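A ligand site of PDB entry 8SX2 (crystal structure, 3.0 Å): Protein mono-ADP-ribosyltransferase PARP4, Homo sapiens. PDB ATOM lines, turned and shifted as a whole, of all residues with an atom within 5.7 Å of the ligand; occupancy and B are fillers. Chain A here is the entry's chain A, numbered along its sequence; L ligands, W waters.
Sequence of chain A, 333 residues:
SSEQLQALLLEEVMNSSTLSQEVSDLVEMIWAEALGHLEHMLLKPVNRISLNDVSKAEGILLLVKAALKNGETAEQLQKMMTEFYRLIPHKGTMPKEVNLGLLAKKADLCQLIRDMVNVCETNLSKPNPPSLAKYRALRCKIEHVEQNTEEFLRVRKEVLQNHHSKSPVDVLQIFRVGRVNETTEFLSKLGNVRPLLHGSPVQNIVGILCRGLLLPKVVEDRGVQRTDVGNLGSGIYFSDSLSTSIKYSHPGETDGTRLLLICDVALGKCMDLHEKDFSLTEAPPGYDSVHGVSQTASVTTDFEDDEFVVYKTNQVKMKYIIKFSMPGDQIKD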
ATOM      1  N   LEU A 197      11.320   9.296  21.889  1.00  0.00           N
ATOM      2  CA  LEU A 197      11.702   9.437  20.498  1.00  0.00           C
ATOM      3  C   LEU A 197      11.131  10.734  19.931  1.00  0.00           C
ATOM      4  O   LEU A 197      10.034  11.148  20.321  1.00  0.00           O
ATOM      5  CB  LEU A 197      11.189   8.218  19.709  1.00  0.00           C
ATOM      6  CG  LEU A 197      12.073   6.971  19.774  1.00  0.00           C
ATOM      7  CD1 LEU A 197      12.278   6.494  21.193  1.00  0.00           C
ATOM      8  CD2 LEU A 197      11.474   5.855  18.931  1.00  0.00           C
ATOM      9  N   HIS A 198      11.869  11.361  19.014  1.00  0.00           N
ATOM     10  CA  HIS A 198      11.417  12.552  18.326  1.00  0.00           C
ATOM     11  C   HIS A 198      11.731  12.432  16.835  1.00  0.00           C
ATOM     12  O   HIS A 198      12.877  12.556  16.429  1.00  0.00           O
ATOM     13  CB  HIS A 198      12.065  13.813  18.907  1.00  0.00           C
ATOM     14  CG  HIS A 198      11.624  15.064  18.225  1.00  0.00           C
ATOM     15  ND1 HIS A 198      10.366  15.590  18.350  1.00  0.00           N
ATOM     16  CD2 HIS A 198      12.288  15.884  17.396  1.00  0.00           C
ATOM     17  CE1 HIS A 198      10.272  16.696  17.625  1.00  0.00           C
ATOM     18  NE2 HIS A 198      11.432  16.892  17.034  1.00  0.00           N
ATOM     19  N   GLY A 199      10.683  12.182  16.032  1.00  0.00           N
ATOM     20  CA  GLY A 199      10.812  12.156  14.582  1.00  0.00           C
ATOM     21  C   GLY A 199      10.813  13.569  13.998  1.00  0.00           C
ATOM     22  O   GLY A 199      10.164  14.470  14.537  1.00  0.00           O
ATOM     23  N   SER A 200      11.545  13.756  12.895  1.00  0.00           N
ATOM     24  CA  SER A 200      11.646  15.058  12.245  1.00  0.00           C
ATOM     25  C   SER A 200      12.192  14.863  10.830  1.00  0.00           C
ATOM     26  O   SER A 200      13.033  14.006  10.608  1.00  0.00           O
ATOM     27  CB  SER A 200      12.513  15.996  13.054  1.00  0.00           C
ATOM     28  OG  SER A 200      12.526  17.294  12.488  1.00  0.00           O
ATOM     29  N   PRO A 201      11.732  15.656   9.827  1.00  0.00           N
ATOM     30  CA  PRO A 201      12.307  15.604   8.484  1.00  0.00           C
ATOM     31  C   PRO A 201      13.795  15.949   8.503  1.00  0.00           C
ATOM     32  O   PRO A 201      14.259  16.660   9.386  1.00  0.00           O
ATOM     33  CB  PRO A 201      11.493  16.618   7.667  1.00  0.00           C
ATOM     34  CG  PRO A 201      10.818  17.498   8.697  1.00  0.00           C
ATOM     35  CD  PRO A 201      10.622  16.626   9.920  1.00  0.00           C
ATOM     36  N   ASN A 204      15.535  19.448   8.849  1.00  0.00           N
ATOM     37  CA  ASN A 204      15.488  20.159  10.108  1.00  0.00           C
ATOM     38  C   ASN A 204      16.714  19.871  10.975  1.00  0.00           C
ATOM     39  O   ASN A 204      16.958  20.565  11.948  1.00  0.00           O
ATOM     40  CB  ASN A 204      14.230  19.801  10.911  1.00  0.00           C
ATOM     41  CG  ASN A 204      12.949  20.271  10.259  1.00  0.00           C
ATOM     42  OD1 ASN A 204      12.957  20.844   9.169  1.00  0.00           O
ATOM     43  ND2 ASN A 204      11.824  20.033  10.916  1.00  0.00           N
ATOM     44  N   GLY A 207      19.484  22.328  11.987  1.00  0.00           N
ATOM     45  CA  GLY A 207      18.928  23.319  12.898  1.00  0.00           C
ATOM     46  C   GLY A 207      18.696  22.752  14.309  1.00  0.00           C
ATOM     47  O   GLY A 207      18.843  23.469  15.291  1.00  0.00           O
ATOM     48  N   ILE A 208      18.330  21.468  14.381  1.00  0.00           N
ATOM     49  CA  ILE A 208      18.117  20.803  15.652  1.00  0.00           C
ATOM     50  C   ILE A 208      19.454  20.590  16.356  1.00  0.00           C
ATOM     51  O   ILE A 208      19.560  20.801  17.561  1.00  0.00           O
ATOM     52  CB  ILE A 208      17.345  19.481  15.453  1.00  0.00           C
ATOM     53  CG1 ILE A 208      15.895  19.744  15.041  1.00  0.00           C
ATOM     54  CG2 ILE A 208      17.422  18.610  16.700  1.00  0.00           C
ATOM     55  CD1 ILE A 208      15.131  18.501  14.629  1.00  0.00           C
ATOM     56  N   ARG A 211      20.902  24.156  17.565  1.00  0.00           N
ATOM     57  CA  ARG A 211      20.229  24.928  18.607  1.00  0.00           C
ATOM     58  C   ARG A 211      19.357  24.051  19.493  1.00  0.00           C
ATOM     59  O   ARG A 211      18.573  24.577  20.276  1.00  0.00           O
ATOM     60  CB  ARG A 211      19.354  26.009  17.959  1.00  0.00           C
ATOM     61  CG  ARG A 211      20.074  26.855  16.921  1.00  0.00           C
ATOM     62  CD  ARG A 211      19.118  27.706  16.107  1.00  0.00           C
ATOM     63  NE  ARG A 211      19.682  27.970  14.803  1.00  0.00           N
ATOM     64  CZ  ARG A 211      19.321  27.349  13.679  1.00  0.00           C
ATOM     65  NH1 ARG A 211      18.335  26.472  13.689  1.00  0.00           N
ATOM     66  NH2 ARG A 211      19.957  27.598  12.552  1.00  0.00           N
ATOM     67  N   GLY A 212      19.494  22.724  19.383  1.00  0.00           N
ATOM     68  CA  GLY A 212      18.617  21.812  20.100  1.00  0.00           C
ATOM     69  C   GLY A 212      17.176  21.906  19.606  1.00  0.00           C
ATOM     70  O   GLY A 212      16.896  22.612  18.638  1.00  0.00           O
ATOM     71  N   LEU A 213      16.279  21.189  20.285  1.00  0.00           N
ATOM     72  CA  LEU A 213      14.849  21.284  20.002  1.00  0.00           C
ATOM     73  C   LEU A 213      14.318  22.577  20.608  1.00  0.00           C
ATOM     74  O   LEU A 213      14.502  22.830  21.799  1.00  0.00           O
ATOM     75  CB  LEU A 213      14.136  20.055  20.582  1.00  0.00           C
ATOM     76  CG  LEU A 213      14.495  18.723  19.940  1.00  0.00           C
ATOM     77  CD1 LEU A 213      13.688  17.583  20.565  1.00  0.00           C
ATOM     78  CD2 LEU A 213      14.266  18.755  18.436  1.00  0.00           C
ATOM     79  N   LEU A 214      13.658  23.395  19.772  1.00  0.00           N
ATOM     80  CA  LEU A 214      13.171  24.701  20.185  1.00  0.00           C
ATOM     81  C   LEU A 214      11.669  24.652  20.401  1.00  0.00           C
ATOM     82  O   LEU A 214      10.996  23.752  19.900  1.00  0.00           O
ATOM     83  CB  LEU A 214      13.535  25.723  19.102  1.00  0.00           C
ATOM     84  CG  LEU A 214      15.027  25.979  18.891  1.00  0.00           C
ATOM     85  CD1 LEU A 214      15.250  27.065  17.853  1.00  0.00           C
ATOM     86  CD2 LEU A 214      15.708  26.347  20.196  1.00  0.00           C
ATOM     87  N   LEU A 215      11.155  25.628  21.155  1.00  0.00           N
ATOM     88  CA  LEU A 215       9.723  25.780  21.399  1.00  0.00           C
ATOM     89  C   LEU A 215       9.072  26.352  20.149  1.00  0.00           C
ATOM     90  O   LEU A 215       9.579  27.310  19.566  1.00  0.00           O
ATOM     91  CB  LEU A 215       9.503  26.709  22.591  1.00  0.00           C
ATOM     92  CG  LEU A 215       9.823  26.124  23.970  1.00  0.00           C
ATOM     93  CD1 LEU A 215       9.586  27.161  25.067  1.00  0.00           C
ATOM     94  CD2 LEU A 215       8.997  24.877  24.229  1.00  0.00           C
ATOM     95  N   PRO A 216       7.922  25.796  19.691  1.00  0.00           N
ATOM     96  CA  PRO A 216       7.174  26.369  18.578  1.00  0.00           C
ATOM     97  C   PRO A 216       6.713  27.800  18.863  1.00  0.00           C
ATOM     98  O   PRO A 216       6.489  28.163  20.017  1.00  0.00           O
ATOM     99  CB  PRO A 216       5.962  25.441  18.405  1.00  0.00           C
ATOM    100  CG  PRO A 216       6.367  24.145  19.091  1.00  0.00           C
ATOM    101  CD  PRO A 216       7.288  24.575  20.218  1.00  0.00           C
ATOM    102  N   VAL A 229      -0.501  24.962  16.245  1.00  0.00           N
ATOM    103  CA  VAL A 229      -0.901  23.877  15.298  1.00  0.00           C
ATOM    104  C   VAL A 229      -0.997  22.553  16.054  1.00  0.00           C
ATOM    105  O   VAL A 229      -1.938  21.786  15.843  1.00  0.00           O
ATOM    106  CB  VAL A 229       0.028  23.778  14.072  1.00  0.00           C
ATOM    107  CG1 VAL A 229       0.029  25.064  13.253  1.00  0.00           C
ATOM    108  CG2 VAL A 229       1.455  23.383  14.431  1.00  0.00           C
ATOM    109  N   GLY A 230      -0.026  22.289  16.945  1.00  0.00           N
ATOM    110  CA  GLY A 230      -0.017  21.081  17.760  1.00  0.00           C
ATOM    111  C   GLY A 230      -1.226  21.009  18.690  1.00  0.00           C
ATOM    112  O   GLY A 230      -1.748  22.035  19.115  1.00  0.00           O
ATOM    113  N   GLY A 235       4.609  23.228  22.460  1.00  0.00           N
ATOM    114  CA  GLY A 235       5.655  22.587  23.234  1.00  0.00           C
ATOM    115  C   GLY A 235       6.465  21.623  22.375  1.00  0.00           C
ATOM    116  O   GLY A 235       6.270  21.549  21.157  1.00  0.00           O
ATOM    117  N   ILE A 236       7.383  20.887  23.027  1.00  0.00           N
ATOM    118  CA  ILE A 236       8.222  19.907  22.347  1.00  0.00           C
ATOM    119  C   ILE A 236       7.617  18.525  22.571  1.00  0.00           C
ATOM    120  O   ILE A 236       7.464  18.103  23.718  1.00  0.00           O
ATOM    121  CB  ILE A 236       9.679  19.996  22.842  1.00  0.00           C
ATOM    122  CG1 ILE A 236      10.165  21.442  22.935  1.00  0.00           C
ATOM    123  CG2 ILE A 236      10.599  19.150  21.961  1.00  0.00           C
ATOM    124  CD1 ILE A 236      11.624  21.577  23.325  1.00  0.00           C
ATOM    125  N   TYR A 237       7.280  17.841  21.476  1.00  0.00           N
ATOM    126  CA  TYR A 237       6.555  16.581  21.535  1.00  0.00           C
ATOM    127  C   TYR A 237       7.515  15.395  21.413  1.00  0.00           C
ATOM    128  O   TYR A 237       8.532  15.483  20.738  1.00  0.00           O
ATOM    129  CB  TYR A 237       5.513  16.504  20.399  1.00  0.00           C
ATOM    130  CG  TYR A 237       4.370  17.479  20.503  1.00  0.00           C
ATOM    131  CD1 TYR A 237       4.590  18.847  20.430  1.00  0.00           C
ATOM    132  CD2 TYR A 237       3.067  17.044  20.661  1.00  0.00           C
ATOM    133  CE1 TYR A 237       3.542  19.757  20.512  1.00  0.00           C
ATOM    134  CE2 TYR A 237       2.010  17.935  20.751  1.00  0.00           C
ATOM    135  CZ  TYR A 237       2.243  19.291  20.675  1.00  0.00           C
ATOM    136  OH  TYR A 237       1.198  20.179  20.758  1.00  0.00           O
ATOM    137  N   PHE A 238       7.146  14.297  22.083  1.00  0.00           N
ATOM    138  CA  PHE A 238       7.876  13.037  21.987  1.00  0.00           C
ATOM    139  C   PHE A 238       6.883  11.880  22.027  1.00  0.00           C
ATOM    140  O   PHE A 238       5.680  12.095  22.203  1.00  0.00           O
ATOM    141  CB  PHE A 238       8.894  12.911  23.131  1.00  0.00           C
ATOM    142  CG  PHE A 238       9.902  14.021  23.213  1.00  0.00           C
ATOM    143  CD1 PHE A 238       9.588  15.231  23.815  1.00  0.00           C
ATOM    144  CD2 PHE A 238      11.164  13.871  22.669  1.00  0.00           C
ATOM    145  CE1 PHE A 238      10.518  16.253  23.889  1.00  0.00           C
ATOM    146  CE2 PHE A 238      12.096  14.898  22.729  1.00  0.00           C
ATOM    147  CZ  PHE A 238      11.774  16.080  23.344  1.00  0.00           C
ATOM    148  N   SER A 239       7.394  10.655  21.867  1.00  0.00           N
ATOM    149  CA  SER A 239       6.571   9.464  21.957  1.00  0.00           C
ATOM    150  C   SER A 239       7.415   8.268  22.414  1.00  0.00           C
ATOM    151  O   SER A 239       8.601   8.190  22.114  1.00  0.00           O
ATOM    152  CB  SER A 239       5.890   9.172  20.646  1.00  0.00           C
ATOM    153  OG  SER A 239       4.983   8.080  20.778  1.00  0.00           O
ATOM    154  N   THR A 244       4.722   5.825  15.878  1.00  0.00           N
ATOM    155  CA  THR A 244       4.148   7.158  15.906  1.00  0.00           C
ATOM    156  C   THR A 244       5.184   8.196  15.453  1.00  0.00           C
ATOM    157  O   THR A 244       4.827   9.194  14.844  1.00  0.00           O
ATOM    158  CB  THR A 244       3.607   7.488  17.297  1.00  0.00           C
ATOM    159  OG1 THR A 244       4.716   7.721  18.171  1.00  0.00           O
ATOM    160  CG2 THR A 244       2.742   6.387  17.874  1.00  0.00           C
ATOM    161  N   SER A 245       6.465   7.943  15.770  1.00  0.00           N
ATOM    162  CA  SER A 245       7.552   8.858  15.465  1.00  0.00           C
ATOM    163  C   SER A 245       7.987   8.724  14.001  1.00  0.00           C
ATOM    164  O   SER A 245       8.655   9.611  13.486  1.00  0.00           O
ATOM    165  CB  SER A 245       8.713   8.649  16.400  1.00  0.00           C
ATOM    166  OG  SER A 245       8.363   9.020  17.726  1.00  0.00           O
ATOM    167  N   TYR A 248       6.266  11.377  11.675  1.00  0.00           N
ATOM    168  CA  TYR A 248       6.802  12.732  11.679  1.00  0.00           C
ATOM    169  C   TYR A 248       8.206  12.756  11.068  1.00  0.00           C
ATOM    170  O   TYR A 248       8.641  13.798  10.584  1.00  0.00           O
ATOM    171  CB  TYR A 248       6.779  13.281  13.100  1.00  0.00           C
ATOM    172  CG  TYR A 248       5.396  13.327  13.714  1.00  0.00           C
ATOM    173  CD1 TYR A 248       4.466  14.261  13.304  1.00  0.00           C
ATOM    174  CD2 TYR A 248       5.010  12.405  14.670  1.00  0.00           C
ATOM    175  CE1 TYR A 248       3.192  14.300  13.834  1.00  0.00           C
ATOM    176  CE2 TYR A 248       3.735  12.422  15.222  1.00  0.00           C
ATOM    177  CZ  TYR A 248       2.824  13.376  14.806  1.00  0.00           C
ATOM    178  OH  TYR A 248       1.560  13.408  15.342  1.00  0.00           O
ATOM    179  N   ASP A 306       0.286   8.065  21.640  1.00  0.00           N
ATOM    180  CA  ASP A 306       0.800   8.577  22.908  1.00  0.00           C
ATOM    181  C   ASP A 306       1.754   9.733  22.638  1.00  0.00           C
ATOM    182  O   ASP A 306       2.807   9.535  22.042  1.00  0.00           O
ATOM    183  CB  ASP A 306       1.494   7.474  23.718  1.00  0.00           C
ATOM    184  CG  ASP A 306       0.565   6.355  24.160  1.00  0.00           C
ATOM    185  OD1 ASP A 306      -0.401   6.646  24.881  1.00  0.00           O
ATOM    186  OD2 ASP A 306       0.831   5.192  23.776  1.00  0.00           O
ATOM    187  N   GLU A 307       1.366  10.932  23.099  1.00  0.00           N
ATOM    188  CA  GLU A 307       2.195  12.118  22.979  1.00  0.00           C
ATOM    189  C   GLU A 307       2.716  12.500  24.363  1.00  0.00           C
ATOM    190  O   GLU A 307       1.969  12.438  25.339  1.00  0.00           O
ATOM    191  CB  GLU A 307       1.391  13.287  22.384  1.00  0.00           C
ATOM    192  CG  GLU A 307       0.772  12.966  21.034  1.00  0.00           C
ATOM    193  CD  GLU A 307      -0.002  14.115  20.400  1.00  0.00           C
ATOM    194  OE1 GLU A 307       0.596  15.187  20.233  1.00  0.00           O
ATOM    195  OE2 GLU A 307      -1.185  13.911  20.072  1.00  0.00           O
HETATM  196  C1  LIG L   1       5.193  12.770  18.389  1.00  0.00           C
HETATM  197  C2  LIG L   1       3.933  13.222  18.693  1.00  0.00           C
HETATM  198  C3  LIG L   1       3.460  14.449  18.200  1.00  0.00           C
HETATM  199  C4  LIG L   1       4.256  15.251  17.392  1.00  0.00           C
HETATM  200  C5  LIG L   1       5.541  14.784  17.079  1.00  0.00           C
HETATM  201  C6  LIG L   1       5.989  13.572  17.581  1.00  0.00           C
HETATM  202  C7  LIG L   1       7.354  13.344  17.094  1.00  0.00           C
HETATM  203  C8  LIG L   1       6.614  15.410  16.239  1.00  0.00           C
HETATM  204  N1  LIG L   1       7.690  14.449  16.376  1.00  0.00           N
HETATM  205  O1  LIG L   1       8.085  12.361  17.281  1.00  0.00           O
HETATM  206  N2  LIG L   1       3.733  16.466  16.903  1.00  0.00           N
HETATM  207  C9  LIG L   1       4.270  17.709  16.932  1.00  0.00           C
HETATM  208  O2  LIG L   1       5.348  17.961  17.462  1.00  0.00           O
HETATM  209  C10 LIG L   1       3.427  18.790  16.281  1.00  0.00           C
HETATM  210  N3  LIG L   1       4.162  19.895  15.679  1.00  0.00           N
HETATM  211  C11 LIG L   1       5.242  19.441  14.796  1.00  0.00           C
HETATM  212  C12 LIG L   1       5.928  20.622  14.130  1.00  0.00           C
HETATM  213  N4  LIG L   1       6.441  21.526  15.155  1.00  0.00           N
HETATM  214  C13 LIG L   1       5.370  21.999  16.031  1.00  0.00           C
HETATM  215  C14 LIG L   1       4.686  20.822  16.684  1.00  0.00           C
HETATM  216  C15 LIG L   1       7.723  21.881  15.336  1.00  0.00           C
HETATM  217  C16 LIG L   1       8.780  21.351  14.418  1.00  0.00           C
HETATM  218  C17 LIG L   1       9.128  19.881  14.658  1.00  0.00           C
HETATM  219  C18 LIG L   1      10.587  19.871  15.160  1.00  0.00           C
HETATM  220  C19 LIG L   1      11.090  21.179  14.553  1.00  0.00           C
HETATM  221  O3  LIG L   1       9.993  22.082  14.626  1.00  0.00           O
HETATM  222  O4  LIG L   1       8.052  22.630  16.256  1.00  0.00           O
HETATM  223  O5  LIG L   1       9.003  19.148  13.458  1.00  0.00           O
HETATM  224  O6  LIG L   1      11.323  18.773  14.690  1.00  0.00           O
HETATM  225  N5  LIG L   1      12.220  21.783  15.248  1.00  0.00           N
HETATM  226  C20 LIG L   1      14.113  22.810  15.720  1.00  0.00           C
HETATM  227  C21 LIG L   1      13.320  22.382  14.672  1.00  0.00           C
HETATM  228  C22 LIG L   1      12.407  21.883  16.601  1.00  0.00           C
HETATM  229  N6  LIG L   1      13.523  22.484  16.934  1.00  0.00           N
HETATM  230  N7  LIG L   1      15.614  23.620  14.092  1.00  0.00           N
HETATM  231  C23 LIG L   1      14.740  23.160  13.180  1.00  0.00           C
HETATM  232  N8  LIG L   1      13.584  22.529  13.363  1.00  0.00           N
HETATM  233  C24 LIG L   1      15.313  23.460  15.399  1.00  0.00           C
HETATM  234  N9  LIG L   1      16.177  23.919  16.310  1.00  0.00           N
HETATM  235  O   HOH W   1       8.375  16.597  13.644  1.00  0.00           O
HETATM  236  O   HOH W   2       0.555  16.560  16.584  1.00  0.00           O
HETATM  237  O   HOH W   3      15.694  26.473  13.198  1.00  0.00           O
HETATM  238  O   HOH W   4       7.934  19.019  18.656  1.00  0.00           O
HETATM  239  O   HOH W   5       9.406  21.561  19.019  1.00  0.00           O
HETATM  240  O   HOH W   6      10.263  24.073  16.801  1.00  0.00           O
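The backbone carbonyl oxygen (O) of Gly 212 sits at hydrogen-bond distance from a nitrogen (N9) of the ligand, at 2.8 Å.
O1 of the ligand is in hydrogen-bond range of N of Gly 199, at 2.9 Å.
O of Gly 199 is in hydrogen-bond range of N1 of the ligand.
O of Gly 207 lies within hydrogen-bond range of N9 of the ligand.
The side-chain hydroxyl (OG) of Ser 200 sits at hydrogen-bond distance from an oxygen (O6) of the ligand (2.9 Å).
N of Leu 214 lies within hydrogen-bond range of N6 of the ligand, at 3.0 Å.
NE2 of His 198 sits at hydrogen-bond distance from O6 of the ligand, at 3.0 Å.
O1 of the ligand is in hydrogen-bond range of OG of Ser 245 (3.4 Å).
The backbone NH (N) of Ile 208 is in hydrogen-bond range of a nitrogen (N7) of the ligand (3.5 Å).
O of Leu 197 touches O1 of the ligand, 3.8 Å away.
Asn 204 touches the ligand (O to C23, 3.6 Å).
Arg 211 touches the ligand.
Leu 213 touches the ligand (CA to N6, 3.6 Å).
CG of Pro 216 touches O4 of the ligand, at 3.6 Å.
Tyr 237 touches the ligand (CD1 to O2, 3.2 Å).
Phe 238 touches the ligand (O to C1, 3.9 Å).
CD2 of Tyr 248 touches C6 of the ligand, at 3.3 Å.
OE1 of Glu 307 touches C3 of the ligand, at 3.6 Å.
Within 4 Å of the ligand: Leu 197, His 198, Gly 199, Ser 200, Asn 204, Gly 207, Ile 208, Arg 211, Gly 212, Leu 213, Leu 214, Pro 216, Tyr 237, Phe 238, Ser 245, Tyr 248 and Glu 307.
The nearest printed residue that does not touch the ligand is Ser 239 (4.3 Å).
Water W1 lies within hydrogen-bond range of O5 of the ligand (2.6 Å) and O of Gly 199 (2.9 Å).
Water W6 bridges an oxygen (O4) of the ligand and the backbone carbonyl oxygen (O) of Leu 214.
Water W3 bridges NH1 of Arg 211 and N7 of the ligand.
Water W4 lies within hydrogen-bond range of O2 of the ligand (3.0 Å) and N of Tyr 237 (3.1 Å).
Water W5 lies within hydrogen-bond range of O of Leu 214 (2.8 Å) and O4 of the ligand (3.3 Å).
The guanidinium group of Arg 211 lies close to the backbone carbonyl oxygen of Gly 207 (3.4 Å).
The side-chain amide nitrogen (ND2) of Asn 204 is in hydrogen-bond range of the side-chain hydroxyl (OG) of Ser 200 (3.2 Å).
ND1 of His 198 lies within hydrogen-bond range of O of Tyr 237 (3.0 Å).
N of Leu 197 is in hydrogen-bond range of O of Ser 239, at 2.9 Å.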
